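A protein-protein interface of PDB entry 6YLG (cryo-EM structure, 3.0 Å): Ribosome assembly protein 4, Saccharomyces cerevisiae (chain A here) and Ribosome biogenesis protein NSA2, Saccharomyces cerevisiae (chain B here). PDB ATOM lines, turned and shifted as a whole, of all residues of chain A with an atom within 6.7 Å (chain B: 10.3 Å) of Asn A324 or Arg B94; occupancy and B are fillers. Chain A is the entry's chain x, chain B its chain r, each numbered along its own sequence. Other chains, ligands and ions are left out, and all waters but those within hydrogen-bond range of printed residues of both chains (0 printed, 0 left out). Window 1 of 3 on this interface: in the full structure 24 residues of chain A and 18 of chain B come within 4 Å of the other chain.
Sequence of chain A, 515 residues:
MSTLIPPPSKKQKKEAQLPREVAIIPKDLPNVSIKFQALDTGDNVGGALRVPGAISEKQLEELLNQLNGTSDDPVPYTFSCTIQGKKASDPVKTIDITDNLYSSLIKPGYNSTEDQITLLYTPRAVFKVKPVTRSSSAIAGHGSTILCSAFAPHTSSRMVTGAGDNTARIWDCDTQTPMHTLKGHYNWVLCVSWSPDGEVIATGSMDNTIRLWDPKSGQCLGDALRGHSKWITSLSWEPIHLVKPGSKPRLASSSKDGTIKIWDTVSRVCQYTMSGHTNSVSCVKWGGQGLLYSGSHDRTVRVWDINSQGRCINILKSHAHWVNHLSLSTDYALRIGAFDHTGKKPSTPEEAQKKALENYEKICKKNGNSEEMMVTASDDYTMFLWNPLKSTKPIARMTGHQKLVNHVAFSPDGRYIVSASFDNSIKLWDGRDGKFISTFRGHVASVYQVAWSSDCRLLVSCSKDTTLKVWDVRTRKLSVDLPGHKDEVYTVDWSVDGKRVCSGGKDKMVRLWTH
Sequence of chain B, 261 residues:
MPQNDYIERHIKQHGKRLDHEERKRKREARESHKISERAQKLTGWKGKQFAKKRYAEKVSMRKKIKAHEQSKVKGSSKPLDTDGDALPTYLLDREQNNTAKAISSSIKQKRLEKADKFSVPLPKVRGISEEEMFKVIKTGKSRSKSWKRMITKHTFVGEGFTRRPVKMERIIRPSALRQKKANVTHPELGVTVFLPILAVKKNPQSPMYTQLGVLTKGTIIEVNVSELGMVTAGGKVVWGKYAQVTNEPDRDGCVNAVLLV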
ATOM      1  N   SER A 282      21.768  12.857 -22.273  1.00  0.00           N
ATOM      2  CA  SER A 282      22.301  13.875 -21.380  1.00  0.00           C
ATOM      3  C   SER A 282      22.411  13.408 -19.939  1.00  0.00           C
ATOM      4  O   SER A 282      23.274  13.908 -19.210  1.00  0.00           O
ATOM      5  CB  SER A 282      21.424  15.119 -21.426  1.00  0.00           C
ATOM      6  OG  SER A 282      21.458  15.705 -22.709  1.00  0.00           O
ATOM      7  N   CYS A 283      21.565  12.475 -19.514  1.00  0.00           N
ATOM      8  CA  CYS A 283      21.538  12.080 -18.114  1.00  0.00           C
ATOM      9  C   CYS A 283      21.153  10.615 -18.006  1.00  0.00           C
ATOM     10  O   CYS A 283      20.387  10.098 -18.820  1.00  0.00           O
ATOM     11  CB  CYS A 283      20.556  12.944 -17.317  1.00  0.00           C
ATOM     12  SG  CYS A 283      20.972  13.135 -15.570  1.00  0.00           S
ATOM     13  N   GLY A 295      17.707  10.350 -19.876  1.00  0.00           N
ATOM     14  CA  GLY A 295      17.154  11.515 -20.542  1.00  0.00           C
ATOM     15  C   GLY A 295      18.102  11.987 -21.633  1.00  0.00           C
ATOM     16  O   GLY A 295      19.299  12.173 -21.392  1.00  0.00           O
ATOM     17  N   SER A 296      17.541  12.190 -22.820  1.00  0.00           N
ATOM     18  CA  SER A 296      18.290  12.419 -24.046  1.00  0.00           C
ATOM     19  C   SER A 296      17.747  13.634 -24.781  1.00  0.00           C
ATOM     20  O   SER A 296      16.709  14.197 -24.428  1.00  0.00           O
ATOM     21  CB  SER A 296      18.224  11.195 -24.958  1.00  0.00           C
ATOM     22  OG  SER A 296      18.449  11.558 -26.307  1.00  0.00           O
ATOM     23  N   HIS A 297      18.463  14.020 -25.836  1.00  0.00           N
ATOM     24  CA  HIS A 297      18.066  15.169 -26.631  1.00  0.00           C
ATOM     25  C   HIS A 297      16.896  14.889 -27.563  1.00  0.00           C
ATOM     26  O   HIS A 297      16.445  15.814 -28.248  1.00  0.00           O
ATOM     27  CB  HIS A 297      19.246  15.690 -27.460  1.00  0.00           C
ATOM     28  CG  HIS A 297      20.285  16.411 -26.663  1.00  0.00           C
ATOM     29  ND1 HIS A 297      21.387  17.001 -27.243  1.00  0.00           N
ATOM     30  CD2 HIS A 297      20.386  16.651 -25.335  1.00  0.00           C
ATOM     31  CE1 HIS A 297      22.126  17.566 -26.306  1.00  0.00           C
ATOM     32  NE2 HIS A 297      21.541  17.367 -25.139  1.00  0.00           N
ATOM     33  N   TRP A 322      14.955  19.802 -25.639  1.00  0.00           N
ATOM     34  CA  TRP A 322      15.845  18.691 -25.377  1.00  0.00           C
ATOM     35  C   TRP A 322      16.211  18.636 -23.895  1.00  0.00           C
ATOM     36  O   TRP A 322      16.320  19.661 -23.219  1.00  0.00           O
ATOM     37  CB  TRP A 322      17.052  18.768 -26.332  1.00  0.00           C
ATOM     38  CG  TRP A 322      18.204  19.735 -26.168  1.00  0.00           C
ATOM     39  CD1 TRP A 322      18.531  20.520 -25.099  1.00  0.00           C
ATOM     40  CD2 TRP A 322      19.204  19.986 -27.161  1.00  0.00           C
ATOM     41  NE1 TRP A 322      19.669  21.239 -25.369  1.00  0.00           N
ATOM     42  CE2 TRP A 322      20.101  20.929 -26.631  1.00  0.00           C
ATOM     43  CE3 TRP A 322      19.423  19.501 -28.453  1.00  0.00           C
ATOM     44  CZ2 TRP A 322      21.198  21.397 -27.347  1.00  0.00           C
ATOM     45  CZ3 TRP A 322      20.509  19.965 -29.162  1.00  0.00           C
ATOM     46  CH2 TRP A 322      21.384  20.904 -28.608  1.00  0.00           C
ATOM     47  N   VAL A 323      16.326  17.415 -23.384  1.00  0.00           N
ATOM     48  CA  VAL A 323      16.264  17.176 -21.946  1.00  0.00           C
ATOM     49  C   VAL A 323      17.649  17.338 -21.336  1.00  0.00           C
ATOM     50  O   VAL A 323      18.657  16.942 -21.931  1.00  0.00           O
ATOM     51  CB  VAL A 323      15.685  15.782 -21.655  1.00  0.00           C
ATOM     52  CG1 VAL A 323      15.856  15.411 -20.193  1.00  0.00           C
ATOM     53  CG2 VAL A 323      14.216  15.732 -22.034  1.00  0.00           C
ATOM     54  N   ASN A 324      17.695  17.929 -20.145  1.00  0.00           N
ATOM     55  CA  ASN A 324      18.931  18.168 -19.417  1.00  0.00           C
ATOM     56  C   ASN A 324      18.728  17.875 -17.935  1.00  0.00           C
ATOM     57  O   ASN A 324      17.820  18.424 -17.305  1.00  0.00           O
ATOM     58  CB  ASN A 324      19.407  19.608 -19.612  1.00  0.00           C
ATOM     59  CG  ASN A 324      19.873  19.878 -21.026  1.00  0.00           C
ATOM     60  OD1 ASN A 324      20.490  19.024 -21.662  1.00  0.00           O
ATOM     61  ND2 ASN A 324      19.587  21.071 -21.524  1.00  0.00           N
ATOM     62  N   HIS A 325      19.582  17.007 -17.394  1.00  0.00           N
ATOM     63  CA  HIS A 325      19.676  16.707 -15.964  1.00  0.00           C
ATOM     64  C   HIS A 325      18.344  16.225 -15.378  1.00  0.00           C
ATOM     65  O   HIS A 325      17.689  16.888 -14.572  1.00  0.00           O
ATOM     66  CB  HIS A 325      20.220  17.890 -15.163  1.00  0.00           C
ATOM     67  CG  HIS A 325      20.873  17.464 -13.890  1.00  0.00           C
ATOM     68  ND1 HIS A 325      20.192  17.389 -12.695  1.00  0.00           N
ATOM     69  CD2 HIS A 325      22.127  17.024 -13.638  1.00  0.00           C
ATOM     70  CE1 HIS A 325      21.009  16.955 -11.752  1.00  0.00           C
ATOM     71  NE2 HIS A 325      22.190  16.727 -12.298  1.00  0.00           N
ATOM     72  N   LEU A 326      17.962  15.040 -15.833  1.00  0.00           N
ATOM     73  CA  LEU A 326      17.103  14.169 -15.045  1.00  0.00           C
ATOM     74  C   LEU A 326      17.613  14.075 -13.609  1.00  0.00           C
ATOM     75  O   LEU A 326      18.820  14.124 -13.355  1.00  0.00           O
ATOM     76  CB  LEU A 326      17.089  12.789 -15.698  1.00  0.00           C
ATOM     77  CG  LEU A 326      16.272  11.614 -15.178  1.00  0.00           C
ATOM     78  CD1 LEU A 326      16.091  10.694 -16.353  1.00  0.00           C
ATOM     79  CD2 LEU A 326      16.952  10.877 -14.035  1.00  0.00           C
ATOM     80  N   SER A 327      16.686  13.930 -12.660  1.00  0.00           N
ATOM     81  CA  SER A 327      17.058  13.707 -11.269  1.00  0.00           C
ATOM     82  C   SER A 327      16.010  12.839 -10.589  1.00  0.00           C
ATOM     83  O   SER A 327      14.876  12.720 -11.062  1.00  0.00           O
ATOM     84  CB  SER A 327      17.220  15.029 -10.515  1.00  0.00           C
ATOM     85  OG  SER A 327      17.452  14.804  -9.136  1.00  0.00           O
ATOM     86  N   VAL A 375      12.203  13.700 -11.670  1.00  0.00           N
ATOM     87  CA  VAL A 375      11.969  15.041 -12.179  1.00  0.00           C
ATOM     88  C   VAL A 375      12.878  15.255 -13.374  1.00  0.00           C
ATOM     89  O   VAL A 375      13.985  14.706 -13.431  1.00  0.00           O
ATOM     90  CB  VAL A 375      12.209  16.114 -11.098  1.00  0.00           C
ATOM     91  CG1 VAL A 375      13.690  16.269 -10.818  1.00  0.00           C
ATOM     92  CG2 VAL A 375      11.598  17.433 -11.521  1.00  0.00           C
ATOM     93  N   THR A 376      12.402  16.046 -14.326  1.00  0.00           N
ATOM     94  CA  THR A 376      13.137  16.336 -15.545  1.00  0.00           C
ATOM     95  C   THR A 376      13.238  17.840 -15.724  1.00  0.00           C
ATOM     96  O   THR A 376      12.489  18.607 -15.122  1.00  0.00           O
ATOM     97  CB  THR A 376      12.462  15.721 -16.771  1.00  0.00           C
ATOM     98  OG1 THR A 376      11.098  16.146 -16.829  1.00  0.00           O
ATOM     99  CG2 THR A 376      12.512  14.209 -16.713  1.00  0.00           C
ATOM    100  N   ALA A 377      14.198  18.249 -16.545  1.00  0.00           N
ATOM    101  CA  ALA A 377      14.374  19.636 -16.938  1.00  0.00           C
ATOM    102  C   ALA A 377      14.660  19.662 -18.428  1.00  0.00           C
ATOM    103  O   ALA A 377      15.289  18.740 -18.954  1.00  0.00           O
ATOM    104  CB  ALA A 377      15.522  20.294 -16.171  1.00  0.00           C
ATOM    105  N   SER A 378      14.196  20.705 -19.115  1.00  0.00           N
ATOM    106  CA  SER A 378      14.496  20.797 -20.538  1.00  0.00           C
ATOM    107  C   SER A 378      14.604  22.250 -20.967  1.00  0.00           C
ATOM    108  O   SER A 378      14.376  23.177 -20.186  1.00  0.00           O
ATOM    109  CB  SER A 378      13.446  20.071 -21.373  1.00  0.00           C
ATOM    110  OG  SER A 378      12.268  20.836 -21.472  1.00  0.00           O
ATOM    111  N   ASP A 379      14.964  22.427 -22.237  1.00  0.00           N
ATOM    112  CA  ASP A 379      15.173  23.731 -22.843  1.00  0.00           C
ATOM    113  C   ASP A 379      13.880  24.381 -23.316  1.00  0.00           C
ATOM    114  O   ASP A 379      13.931  25.452 -23.928  1.00  0.00           O
ATOM    115  CB  ASP A 379      16.155  23.610 -24.009  1.00  0.00           C
ATOM    116  CG  ASP A 379      17.568  23.327 -23.548  1.00  0.00           C
ATOM    117  OD1 ASP A 379      17.743  22.960 -22.368  1.00  0.00           O
ATOM    118  OD2 ASP A 379      18.502  23.473 -24.363  1.00  0.00           O
ATOM    119  N   LEU A 404      16.104  28.561 -20.047  1.00  0.00           N
ATOM    120  CA  LEU A 404      16.076  27.120 -19.875  1.00  0.00           C
ATOM    121  C   LEU A 404      16.552  26.707 -18.489  1.00  0.00           C
ATOM    122  O   LEU A 404      17.143  27.487 -17.736  1.00  0.00           O
ATOM    123  CB  LEU A 404      16.945  26.441 -20.928  1.00  0.00           C
ATOM    124  CG  LEU A 404      18.424  26.813 -20.927  1.00  0.00           C
ATOM    125  CD1 LEU A 404      19.261  25.684 -20.360  1.00  0.00           C
ATOM    126  CD2 LEU A 404      18.866  27.156 -22.331  1.00  0.00           C
ATOM    127  N   VAL A 405      16.280  25.447 -18.165  1.00  0.00           N
ATOM    128  CA  VAL A 405      16.734  24.811 -16.938  1.00  0.00           C
ATOM    129  C   VAL A 405      17.929  23.937 -17.281  1.00  0.00           C
ATOM    130  O   VAL A 405      17.886  23.165 -18.246  1.00  0.00           O
ATOM    131  CB  VAL A 405      15.614  23.977 -16.293  1.00  0.00           C
ATOM    132  CG1 VAL A 405      15.912  23.723 -14.832  1.00  0.00           C
ATOM    133  CG2 VAL A 405      14.273  24.663 -16.450  1.00  0.00           C
ATOM    134  N   ASN A 406      18.992  24.062 -16.491  1.00  0.00           N
ATOM    135  CA  ASN A 406      20.236  23.336 -16.710  1.00  0.00           C
ATOM    136  C   ASN A 406      20.502  22.281 -15.654  1.00  0.00           C
ATOM    137  O   ASN A 406      21.165  21.282 -15.949  1.00  0.00           O
ATOM    138  CB  ASN A 406      21.412  24.313 -16.736  1.00  0.00           C
ATOM    139  CG  ASN A 406      22.677  23.686 -17.274  1.00  0.00           C
ATOM    140  OD1 ASN A 406      22.703  23.171 -18.390  1.00  0.00           O
ATOM    141  ND2 ASN A 406      23.736  23.722 -16.478  1.00  0.00           N
ATOM    142  N   HIS A 407      20.001  22.478 -14.438  1.00  0.00           N
ATOM    143  CA  HIS A 407      20.285  21.569 -13.340  1.00  0.00           C
ATOM    144  C   HIS A 407      19.087  21.528 -12.406  1.00  0.00           C
ATOM    145  O   HIS A 407      18.421  22.546 -12.183  1.00  0.00           O
ATOM    146  CB  HIS A 407      21.540  22.004 -12.581  1.00  0.00           C
ATOM    147  CG  HIS A 407      22.095  20.953 -11.675  1.00  0.00           C
ATOM    148  ND1 HIS A 407      21.970  21.008 -10.303  1.00  0.00           N
ATOM    149  CD2 HIS A 407      22.798  19.830 -11.944  1.00  0.00           C
ATOM    150  CE1 HIS A 407      22.562  19.954  -9.768  1.00  0.00           C
ATOM    151  NE2 HIS A 407      23.071  19.223 -10.742  1.00  0.00           N
ATOM    152  N   VAL A 408      18.826  20.337 -11.875  1.00  0.00           N
ATOM    153  CA  VAL A 408      17.740  20.087 -10.944  1.00  0.00           C
ATOM    154  C   VAL A 408      18.320  19.335  -9.759  1.00  0.00           C
ATOM    155  O   VAL A 408      19.370  18.694  -9.854  1.00  0.00           O
ATOM    156  CB  VAL A 408      16.593  19.281 -11.586  1.00  0.00           C
ATOM    157  CG1 VAL A 408      15.301  19.458 -10.796  1.00  0.00           C
ATOM    158  CG2 VAL A 408      16.414  19.678 -13.037  1.00  0.00           C
ATOM    159  N   PHE A 422      18.972  29.549 -16.539  1.00  0.00           N
ATOM    160  CA  PHE A 422      19.795  30.547 -17.209  1.00  0.00           C
ATOM    161  C   PHE A 422      19.209  31.951 -17.139  1.00  0.00           C
ATOM    162  O   PHE A 422      19.834  32.886 -17.650  1.00  0.00           O
ATOM    163  CB  PHE A 422      19.991  30.156 -18.682  1.00  0.00           C
ATOM    164  CG  PHE A 422      21.102  29.160 -18.928  1.00  0.00           C
ATOM    165  CD1 PHE A 422      21.518  28.270 -17.950  1.00  0.00           C
ATOM    166  CD2 PHE A 422      21.724  29.114 -20.162  1.00  0.00           C
ATOM    167  CE1 PHE A 422      22.532  27.376 -18.202  1.00  0.00           C
ATOM    168  CE2 PHE A 422      22.734  28.215 -20.412  1.00  0.00           C
ATOM    169  CZ  PHE A 422      23.136  27.347 -19.432  1.00  0.00           C
ATOM    170  N   LEU B  87      34.850  22.895 -22.351  1.00  0.00           N
ATOM    171  CA  LEU B  87      33.563  23.194 -21.747  1.00  0.00           C
ATOM    172  C   LEU B  87      33.004  21.931 -21.113  1.00  0.00           C
ATOM    173  O   LEU B  87      33.386  20.821 -21.496  1.00  0.00           O
ATOM    174  CB  LEU B  87      32.568  23.733 -22.786  1.00  0.00           C
ATOM    175  CG  LEU B  87      33.030  24.908 -23.644  1.00  0.00           C
ATOM    176  CD1 LEU B  87      32.141  25.031 -24.863  1.00  0.00           C
ATOM    177  CD2 LEU B  87      33.033  26.194 -22.839  1.00  0.00           C
ATOM    178  N   PRO B  88      32.097  22.054 -20.140  1.00  0.00           N
ATOM    179  CA  PRO B  88      31.511  20.850 -19.543  1.00  0.00           C
ATOM    180  C   PRO B  88      30.453  20.232 -20.442  1.00  0.00           C
ATOM    181  O   PRO B  88      30.181  20.684 -21.557  1.00  0.00           O
ATOM    182  CB  PRO B  88      30.897  21.341 -18.228  1.00  0.00           C
ATOM    183  CG  PRO B  88      31.346  22.728 -18.060  1.00  0.00           C
ATOM    184  CD  PRO B  88      31.663  23.256 -19.407  1.00  0.00           C
ATOM    185  N   THR B  89      29.845  19.171 -19.911  1.00  0.00           N
ATOM    186  CA  THR B  89      28.879  18.387 -20.673  1.00  0.00           C
ATOM    187  C   THR B  89      27.678  19.228 -21.085  1.00  0.00           C
ATOM    188  O   THR B  89      27.120  19.042 -22.173  1.00  0.00           O
ATOM    189  CB  THR B  89      28.429  17.185 -19.844  1.00  0.00           C
ATOM    190  OG1 THR B  89      27.823  17.641 -18.629  1.00  0.00           O
ATOM    191  CG2 THR B  89      29.616  16.308 -19.503  1.00  0.00           C
ATOM    192  N   TYR B  90      27.273  20.168 -20.231  1.00  0.00           N
ATOM    193  CA  TYR B  90      26.023  20.886 -20.455  1.00  0.00           C
ATOM    194  C   TYR B  90      26.190  22.128 -21.320  1.00  0.00           C
ATOM    195  O   TYR B  90      25.220  22.526 -21.975  1.00  0.00           O
ATOM    196  CB  TYR B  90      25.359  21.262 -19.123  1.00  0.00           C
ATOM    197  CG  TYR B  90      26.253  21.882 -18.069  1.00  0.00           C
ATOM    198  CD1 TYR B  90      26.765  23.156 -18.227  1.00  0.00           C
ATOM    199  CD2 TYR B  90      26.573  21.188 -16.913  1.00  0.00           C
ATOM    200  CE1 TYR B  90      27.574  23.723 -17.266  1.00  0.00           C
ATOM    201  CE2 TYR B  90      27.380  21.747 -15.948  1.00  0.00           C
ATOM    202  CZ  TYR B  90      27.878  23.013 -16.131  1.00  0.00           C
ATOM    203  OH  TYR B  90      28.683  23.574 -15.171  1.00  0.00           O
ATOM    204  N   LEU B  91      27.375  22.744 -21.348  1.00  0.00           N
ATOM    205  CA  LEU B  91      27.655  23.813 -22.300  1.00  0.00           C
ATOM    206  C   LEU B  91      28.278  23.310 -23.592  1.00  0.00           C
ATOM    207  O   LEU B  91      28.409  24.093 -24.538  1.00  0.00           O
ATOM    208  CB  LEU B  91      28.581  24.867 -21.685  1.00  0.00           C
ATOM    209  CG  LEU B  91      27.972  25.801 -20.636  1.00  0.00           C
ATOM    210  CD1 LEU B  91      29.049  26.662 -20.001  1.00  0.00           C
ATOM    211  CD2 LEU B  91      26.871  26.666 -21.230  1.00  0.00           C
ATOM    212  N   LEU B  92      28.674  22.042 -23.656  1.00  0.00           N
ATOM    213  CA  LEU B  92      28.915  21.428 -24.949  1.00  0.00           C
ATOM    214  C   LEU B  92      27.594  21.302 -25.697  1.00  0.00           C
ATOM    215  O   LEU B  92      26.514  21.458 -25.122  1.00  0.00           O
ATOM    216  CB  LEU B  92      29.565  20.054 -24.795  1.00  0.00           C
ATOM    217  CG  LEU B  92      31.054  20.028 -24.458  1.00  0.00           C
ATOM    218  CD1 LEU B  92      31.395  18.721 -23.782  1.00  0.00           C
ATOM    219  CD2 LEU B  92      31.904  20.227 -25.701  1.00  0.00           C
ATOM    220  N   ASP B  93      27.689  21.006 -26.994  1.00  0.00           N
ATOM    221  CA  ASP B  93      26.469  20.861 -27.798  1.00  0.00           C
ATOM    222  C   ASP B  93      25.802  22.211 -28.078  1.00  0.00           C
ATOM    223  O   ASP B  93      24.652  22.260 -28.522  1.00  0.00           O
ATOM    224  CB  ASP B  93      25.468  19.892 -27.136  1.00  0.00           C
ATOM    225  CG  ASP B  93      25.374  18.557 -27.849  1.00  0.00           C
ATOM    226  OD1 ASP B  93      25.545  18.541 -29.086  1.00  0.00           O
ATOM    227  OD2 ASP B  93      25.165  17.518 -27.186  1.00  0.00           O
ATOM    228  N   ARG B  94      26.460  23.321 -27.740  1.00  0.00           N
ATOM    229  CA  ARG B  94      25.856  24.648 -27.833  1.00  0.00           C
ATOM    230  C   ARG B  94      26.405  25.414 -29.030  1.00  0.00           C
ATOM    231  O   ARG B  94      26.455  26.643 -29.021  1.00  0.00           O
ATOM    232  CB  ARG B  94      26.106  25.444 -26.552  1.00  0.00           C
ATOM    233  CG  ARG B  94      25.600  24.772 -25.290  1.00  0.00           C
ATOM    234  CD  ARG B  94      24.088  24.722 -25.239  1.00  0.00           C
ATOM    235  NE  ARG B  94      23.612  24.244 -23.944  1.00  0.00           N
ATOM    236  CZ  ARG B  94      22.335  24.184 -23.573  1.00  0.00           C
ATOM    237  NH1 ARG B  94      21.360  24.575 -24.384  1.00  0.00           N
ATOM    238  NH2 ARG B  94      22.030  23.726 -22.370  1.00  0.00           N
ATOM    239  N   GLU B 188      17.760  22.966 -33.938  1.00  0.00           N
ATOM    240  CA  GLU B 188      17.983  22.076 -32.818  1.00  0.00           C
ATOM    241  C   GLU B 188      17.084  20.849 -32.958  1.00  0.00           C
ATOM    242  O   GLU B 188      16.102  20.848 -33.698  1.00  0.00           O
ATOM    243  CB  GLU B 188      17.708  22.801 -31.503  1.00  0.00           C
ATOM    244  CG  GLU B 188      18.603  24.007 -31.251  1.00  0.00           C
ATOM    245  CD  GLU B 188      17.913  25.087 -30.436  1.00  0.00           C
ATOM    246  OE1 GLU B 188      18.137  25.148 -29.210  1.00  0.00           O
ATOM    247  OE2 GLU B 188      17.145  25.877 -31.026  1.00  0.00           O
ATOM    248  N   LEU B 189      17.466  19.781 -32.253  1.00  0.00           N
ATOM    249  CA  LEU B 189      16.748  18.507 -32.202  1.00  0.00           C
ATOM    250  C   LEU B 189      16.904  17.656 -33.460  1.00  0.00           C
ATOM    251  O   LEU B 189      16.525  16.481 -33.446  1.00  0.00           O
ATOM    252  CB  LEU B 189      15.247  18.716 -31.954  1.00  0.00           C
ATOM    253  CG  LEU B 189      14.784  19.681 -30.863  1.00  0.00           C
ATOM    254  CD1 LEU B 189      13.339  20.085 -31.102  1.00  0.00           C
ATOM    255  CD2 LEU B 189      14.942  19.036 -29.506  1.00  0.00           C
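The side-chain carboxylate (OD2) of Asp A379 is in salt-bridge range of the guanidinium group (NH1) of Arg B94 (3.1 Å).
O of Tyr B90 is in hydrogen-bond range of NE of Arg B94, 3.1 Å away.
A ring nitrogen (NE2) of His A297 sits at hydrogen-bond distance from the side-chain hydroxyl of Ser A282 (2.9 Å).
The indole nitrogen (NE1) of Trp A322 is in hydrogen-bond range of the side-chain carboxylate (OD2) of Asp A379, at 2.7 Å.
The backbone carbonyl oxygen of Ala A377 sits at hydrogen-bond distance from the backbone NH of Asn A324, 2.8 Å away.
The side-chain carboxylate (OD1) of Asp A379 sits at hydrogen-bond distance from the side-chain amide nitrogen (ND2) of Asn A324 (2.8 Å).
O of Leu A404 is in hydrogen-bond range of N of Phe A422 (3.0 Å).
OD2 of Asp B93 touches CE1 of His A297 (3.2 Å).
His A297 touches Leu B189.
Trp A322 touches Asp B93 (CH2 to O, 3.5 Å).
NE1 of Trp A322 touches NH1 of Arg B94 (3.9 Å).
Trp A322 touches Leu B189.
ND2 of Asn A324 touches NH2 of Arg B94 (3.7 Å).
NH2 of Arg B94 touches CD1 of Leu A404, at 3.9 Å.
Tyr B90 touches Asn A406.
Asn A324 touches just one residue of chain B: Arg B94.
Of chain A, only Trp A322 (3.9 Å), Asn A324 (3.7 Å), Asp A379 (3.1 Å) and Leu A404 (3.9 Å) come within 4 Å of Arg B94.
No residue of chain B comes within 4 Å of Val A323.
Asn A406 touches just one residue of chain B: Tyr B90.
Of the printed residues of chain B, Leu A404 touches Arg B94 (3.9 Å).
Of the printed residues of chain A, Leu B189 touches His A297 (3.8 Å) and Trp A322 (3.8 Å).
Printed residues of chain A within 4 Å of Asp B93: His A297 (3.2 Å) and Trp A322 (3.5 Å).
The nearest residue of chain A that does not touch Arg B94 is Asn A406 (4.1 Å).
The nearest printed residue of chain A that does not touch Leu B189 is Val A323 (6.5 Å).
Of the 10 printed residues of chain B, 4 touch a printed residue of chain A.
Hydrophobic or aromatic side chains of chain B that line the printed part of chain A: Tyr B90 and Leu B189.
Of the 22 printed residues of chain A, 6 touch a printed residue of chain B.
Hydrophobic or aromatic side chains of chain A that line the printed part of chain B: His A297, Trp A322 and Leu A404.
Among the printed residues, 9 pairs touch across the chains.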
